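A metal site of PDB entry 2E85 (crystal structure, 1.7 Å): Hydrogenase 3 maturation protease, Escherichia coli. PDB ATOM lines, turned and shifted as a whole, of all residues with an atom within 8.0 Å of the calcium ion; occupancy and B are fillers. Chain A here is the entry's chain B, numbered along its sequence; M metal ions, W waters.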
ATOM      1  N   VAL A  11     -20.559 -16.090 -16.820  1.00  0.00           N
ATOM      2  CA  VAL A  11     -20.271 -17.431 -17.313  1.00  0.00           C
ATOM      3  C   VAL A  11     -21.373 -17.919 -18.262  1.00  0.00           C
ATOM      4  O   VAL A  11     -22.541 -17.704 -17.996  1.00  0.00           O
ATOM      5  CB  VAL A  11     -20.118 -18.465 -16.103  1.00  0.00           C
ATOM      6  CG1 VAL A  11     -19.898 -19.900 -16.597  1.00  0.00           C
ATOM      7  CG2 VAL A  11     -18.988 -18.026 -15.133  1.00  0.00           C
ATOM      8  N   GLY A  12     -20.979 -18.571 -19.359  1.00  0.00           N
ATOM      9  CA  GLY A  12     -21.957 -19.155 -20.260  1.00  0.00           C
ATOM     10  C   GLY A  12     -21.483 -19.252 -21.693  1.00  0.00           C
ATOM     11  O   GLY A  12     -20.353 -18.924 -22.022  1.00  0.00           O
ATOM     12  N   ASN A  13     -22.385 -19.716 -22.549  1.00  0.00           N
ATOM     13  CA  ASN A  13     -22.035 -19.965 -23.951  1.00  0.00           C
ATOM     14  C   ASN A  13     -23.198 -19.490 -24.798  1.00  0.00           C
ATOM     15  O   ASN A  13     -24.298 -20.035 -24.670  1.00  0.00           O
ATOM     16  CB  ASN A  13     -21.765 -21.462 -24.130  1.00  0.00           C
ATOM     17  CG  ASN A  13     -21.253 -21.830 -25.522  1.00  0.00           C
ATOM     18  OD1 ASN A  13     -21.361 -21.060 -26.476  1.00  0.00           O
ATOM     19  ND2 ASN A  13     -20.662 -23.021 -25.622  1.00  0.00           N
ATOM     20  N   MET A  16     -25.333 -21.825 -26.867  1.00  0.00           N
ATOM     21  CA  MET A  16     -26.047 -22.897 -26.165  1.00  0.00           C
ATOM     22  C   MET A  16     -27.398 -22.429 -25.592  1.00  0.00           C
ATOM     23  O   MET A  16     -27.779 -22.794 -24.465  1.00  0.00           O
ATOM     24  CB  MET A  16     -25.147 -23.560 -25.123  1.00  0.00           C
ATOM     25  CG  MET A  16     -24.009 -24.411 -25.710  1.00  0.00           C
ATOM     26  SD  MET A  16     -24.539 -25.955 -26.587  1.00  0.00           S
ATOM     27  CE  MET A  16     -24.941 -26.973 -25.237  1.00  0.00           C
ATOM     28  N   ASP A  18     -30.338 -20.814 -23.782  1.00  0.00           N
ATOM     29  CA  ASP A  18     -30.447 -20.079 -22.532  1.00  0.00           C
ATOM     30  C   ASP A  18     -29.150 -20.073 -21.714  1.00  0.00           C
ATOM     31  O   ASP A  18     -29.015 -19.223 -20.824  1.00  0.00           O
ATOM     32  CB  ASP A  18     -31.624 -20.597 -21.678  1.00  0.00           C
ATOM     33  CG  ASP A  18     -32.989 -20.182 -22.223  1.00  0.00           C
ATOM     34  OD1 ASP A  18     -33.057 -19.161 -22.946  1.00  0.00           O
ATOM     35  OD2 ASP A  18     -33.986 -20.906 -21.908  1.00  0.00           O
ATOM     36  N   ASP A  19     -28.219 -20.978 -22.011  1.00  0.00           N
ATOM     37  CA  ASP A  19     -26.877 -20.889 -21.385  1.00  0.00           C
ATOM     38  C   ASP A  19     -26.146 -19.589 -21.746  1.00  0.00           C
ATOM     39  O   ASP A  19     -25.080 -19.297 -21.156  1.00  0.00           O
ATOM     40  CB  ASP A  19     -26.000 -22.082 -21.745  1.00  0.00           C
ATOM     41  CG  ASP A  19     -24.819 -22.198 -20.791  1.00  0.00           C
ATOM     42  OD1 ASP A  19     -25.094 -22.091 -19.573  1.00  0.00           O
ATOM     43  OD2 ASP A  19     -23.668 -22.315 -21.239  1.00  0.00           O
ATOM     44  N   GLY A  20     -26.689 -18.832 -22.705  1.00  0.00           N
ATOM     45  CA  GLY A  20     -26.145 -17.535 -23.102  1.00  0.00           C
ATOM     46  C   GLY A  20     -26.413 -16.386 -22.141  1.00  0.00           C
ATOM     47  O   GLY A  20     -26.049 -15.250 -22.419  1.00  0.00           O
ATOM     48  N   ALA A  21     -27.053 -16.679 -21.005  1.00  0.00           N
ATOM     49  CA  ALA A  21     -27.492 -15.602 -20.115  1.00  0.00           C
ATOM     50  C   ALA A  21     -26.296 -14.754 -19.667  1.00  0.00           C
ATOM     51  O   ALA A  21     -26.356 -13.513 -19.672  1.00  0.00           O
ATOM     52  CB  ALA A  21     -28.220 -16.164 -18.939  1.00  0.00           C
ATOM     53  N   GLY A  22     -25.213 -15.435 -19.310  1.00  0.00           N
ATOM     54  CA  GLY A  22     -24.011 -14.727 -18.834  1.00  0.00           C
ATOM     55  C   GLY A  22     -23.411 -13.818 -19.919  1.00  0.00           C
ATOM     56  O   GLY A  22     -23.235 -12.643 -19.705  1.00  0.00           O
ATOM     57  N   PRO A  23     -23.058 -14.370 -21.093  1.00  0.00           N
ATOM     58  CA  PRO A  23     -22.627 -13.527 -22.220  1.00  0.00           C
ATOM     59  C   PRO A  23     -23.586 -12.395 -22.566  1.00  0.00           C
ATOM     60  O   PRO A  23     -23.133 -11.283 -22.854  1.00  0.00           O
ATOM     61  CB  PRO A  23     -22.494 -14.529 -23.378  1.00  0.00           C
ATOM     62  CG  PRO A  23     -22.186 -15.842 -22.675  1.00  0.00           C
ATOM     63  CD  PRO A  23     -22.875 -15.818 -21.362  1.00  0.00           C
ATOM     64  N   GLY A  43     -17.112 -16.743 -20.751  1.00  0.00           N
ATOM     65  CA  GLY A  43     -17.362 -17.882 -21.625  1.00  0.00           C
ATOM     66  C   GLY A  43     -17.699 -19.165 -20.851  1.00  0.00           C
ATOM     67  O   GLY A  43     -18.214 -19.118 -19.734  1.00  0.00           O
ATOM     68  N   SER A  44     -17.362 -20.289 -21.471  1.00  0.00           N
ATOM     69  CA  SER A  44     -17.787 -21.608 -21.045  1.00  0.00           C
ATOM     70  C   SER A  44     -17.256 -22.084 -19.704  1.00  0.00           C
ATOM     71  O   SER A  44     -17.968 -22.804 -18.986  1.00  0.00           O
ATOM     72  CB  SER A  44     -17.420 -22.639 -22.119  1.00  0.00           C
ATOM     73  OG  SER A  44     -18.111 -22.349 -23.302  1.00  0.00           O
ATOM     74  N   VAL A  64     -22.303 -14.605 -12.380  1.00  0.00           N
ATOM     75  CA  VAL A  64     -23.635 -14.820 -12.929  1.00  0.00           C
ATOM     76  C   VAL A  64     -23.562 -15.933 -13.980  1.00  0.00           C
ATOM     77  O   VAL A  64     -22.760 -15.864 -14.910  1.00  0.00           O
ATOM     78  CB  VAL A  64     -24.183 -13.536 -13.607  1.00  0.00           C
ATOM     79  CG1 VAL A  64     -25.465 -13.840 -14.448  1.00  0.00           C
ATOM     80  CG2 VAL A  64     -24.386 -12.389 -12.557  1.00  0.00           C
ATOM     81  N   ASP A  65     -24.428 -16.927 -13.829  1.00  0.00           N
ATOM     82  CA  ASP A  65     -24.373 -18.109 -14.693  1.00  0.00           C
ATOM     83  C   ASP A  65     -25.773 -18.700 -14.812  1.00  0.00           C
ATOM     84  O   ASP A  65     -26.482 -18.796 -13.818  1.00  0.00           O
ATOM     85  CB  ASP A  65     -23.434 -19.151 -14.069  1.00  0.00           C
ATOM     86  CG  ASP A  65     -23.115 -20.326 -15.006  1.00  0.00           C
ATOM     87  OD1 ASP A  65     -23.492 -20.306 -16.179  1.00  0.00           O
ATOM     88  OD2 ASP A  65     -22.422 -21.265 -14.569  1.00  0.00           O
ATOM     89  N   ALA A  66     -26.162 -19.110 -16.011  1.00  0.00           N
ATOM     90  CA  ALA A  66     -27.348 -19.888 -16.188  1.00  0.00           C
ATOM     91  C   ALA A  66     -27.062 -21.272 -15.536  1.00  0.00           C
ATOM     92  O   ALA A  66     -26.040 -21.898 -15.834  1.00  0.00           O
ATOM     93  CB  ALA A  66     -27.632 -20.081 -17.684  1.00  0.00           C
ATOM     94  N   THR A  67     -27.970 -21.741 -14.685  1.00  0.00           N
ATOM     95  CA  THR A  67     -27.722 -22.890 -13.835  1.00  0.00           C
ATOM     96  C   THR A  67     -29.058 -23.611 -13.621  1.00  0.00           C
ATOM     97  O   THR A  67     -30.005 -22.980 -13.226  1.00  0.00           O
ATOM     98  CB  THR A  67     -27.246 -22.406 -12.423  1.00  0.00           C
ATOM     99  OG1 THR A  67     -26.011 -21.670 -12.540  1.00  0.00           O
ATOM    100  CG2 THR A  67     -27.089 -23.530 -11.459  1.00  0.00           C
ATOM    101  N   ASP A  68     -29.124 -24.928 -13.856  1.00  0.00           N
ATOM    102  CA  ASP A  68     -30.383 -25.639 -13.578  1.00  0.00           C
ATOM    103  C   ASP A  68     -30.515 -25.791 -12.060  1.00  0.00           C
ATOM    104  O   ASP A  68     -29.626 -26.363 -11.396  1.00  0.00           O
ATOM    105  CB  ASP A  68     -30.449 -27.003 -14.299  1.00  0.00           C
ATOM    106  CG  ASP A  68     -31.772 -27.749 -14.028  1.00  0.00           C
ATOM    107  OD1 ASP A  68     -32.819 -27.115 -13.782  1.00  0.00           O
ATOM    108  OD2 ASP A  68     -31.761 -29.008 -14.087  1.00  0.00           O
ATOM    109  N   MET A  90     -20.774 -28.668 -11.058  1.00  0.00           N
ATOM    110  CA  MET A  90     -19.500 -28.855 -11.786  1.00  0.00           C
ATOM    111  C   MET A  90     -19.263 -27.804 -12.873  1.00  0.00           C
ATOM    112  O   MET A  90     -20.188 -27.271 -13.472  1.00  0.00           O
ATOM    113  CB  MET A  90     -19.443 -30.249 -12.425  1.00  0.00           C
ATOM    114  CG  MET A  90     -19.756 -31.429 -11.515  1.00  0.00           C
ATOM    115  SD  MET A  90     -18.395 -31.761 -10.359  1.00  0.00           S
ATOM    116  CE  MET A  90     -19.120 -31.446  -8.812  1.00  0.00           C
ATOM    117  N   PHE A 113     -22.631 -15.855  -5.761  1.00  0.00           N
ATOM    118  CA  PHE A 113     -22.904 -16.662  -6.943  1.00  0.00           C
ATOM    119  C   PHE A 113     -24.373 -16.555  -7.239  1.00  0.00           C
ATOM    120  O   PHE A 113     -25.203 -17.014  -6.427  1.00  0.00           O
ATOM    121  CB  PHE A 113     -22.577 -18.147  -6.713  1.00  0.00           C
ATOM    122  CG  PHE A 113     -22.768 -18.959  -7.952  1.00  0.00           C
ATOM    123  CD1 PHE A 113     -21.721 -19.097  -8.844  1.00  0.00           C
ATOM    124  CD2 PHE A 113     -24.031 -19.481  -8.287  1.00  0.00           C
ATOM    125  CE1 PHE A 113     -21.890 -19.790 -10.023  1.00  0.00           C
ATOM    126  CE2 PHE A 113     -24.205 -20.192  -9.482  1.00  0.00           C
ATOM    127  CZ  PHE A 113     -23.129 -20.328 -10.335  1.00  0.00           C
ATOM    128  N   ILE A 116     -29.329 -18.198 -12.795  1.00  0.00           N
ATOM    129  CA  ILE A 116     -30.551 -17.898 -13.516  1.00  0.00           C
ATOM    130  C   ILE A 116     -30.984 -19.221 -14.118  1.00  0.00           C
ATOM    131  O   ILE A 116     -30.177 -19.884 -14.827  1.00  0.00           O
ATOM    132  CB  ILE A 116     -30.295 -16.955 -14.710  1.00  0.00           C
ATOM    133  CG1 ILE A 116     -29.803 -15.594 -14.227  1.00  0.00           C
ATOM    134  CG2 ILE A 116     -31.535 -16.836 -15.619  1.00  0.00           C
ATOM    135  CD1 ILE A 116     -29.189 -14.711 -15.307  1.00  0.00           C
ATOM    136  N   PRO A 118     -32.267 -21.682 -16.683  1.00  0.00           N
ATOM    137  CA  PRO A 118     -32.564 -21.795 -18.107  1.00  0.00           C
ATOM    138  C   PRO A 118     -33.765 -22.672 -18.370  1.00  0.00           C
ATOM    139  O   PRO A 118     -34.206 -23.467 -17.504  1.00  0.00           O
ATOM    140  CB  PRO A 118     -31.325 -22.473 -18.677  1.00  0.00           C
ATOM    141  CG  PRO A 118     -30.863 -23.359 -17.593  1.00  0.00           C
ATOM    142  CD  PRO A 118     -31.107 -22.512 -16.300  1.00  0.00           C
ATOM    143  N   VAL A 121     -31.432 -25.517 -23.424  1.00  0.00           N
ATOM    144  CA  VAL A 121     -29.976 -25.433 -23.565  1.00  0.00           C
ATOM    145  C   VAL A 121     -29.570 -26.436 -24.608  1.00  0.00           C
ATOM    146  O   VAL A 121     -29.744 -27.630 -24.421  1.00  0.00           O
ATOM    147  CB  VAL A 121     -29.247 -25.734 -22.225  1.00  0.00           C
ATOM    148  CG1 VAL A 121     -27.704 -25.777 -22.410  1.00  0.00           C
ATOM    149  CG2 VAL A 121     -29.648 -24.713 -21.115  1.00  0.00           C
HETATM  150 CA    CA M   1     -24.031 -22.131 -17.488  1.00  0.00          CA
HETATM  151  O   HOH W   1     -24.658 -24.269 -17.767  1.00  0.00           O
HETATM  152  O   HOH W   2     -23.077 -23.536 -15.787  1.00  0.00           O
HETATM  153  O   HOH W   3     -21.647 -22.659 -17.414  1.00  0.00           O
HETATM  154  O   HOH W   4     -27.144 -23.387 -18.368  1.00  0.00           O
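The backbone carbonyl oxygen (O) of Asp 65 sits at hydrogen-bond distance from the side-chain hydroxyl (OG1) of Thr 67 (3.2 Å). The backbone carbonyl oxygen (O) of Asp 65 lies within hydrogen-bond range of the backbone NH (N) of Ile 116 (3.1 Å). The backbone carbonyl oxygen (O) of Asp 19 lies within hydrogen-bond range of the backbone NH (N) of Asn 13 (3.1 Å).
The calcium ion is bound by water W1, OD1 of Asp 65, OD1 of Asp 19, water W2, water W3 and O of Ala 66. The calcium ion has six donor atoms within binding distance.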
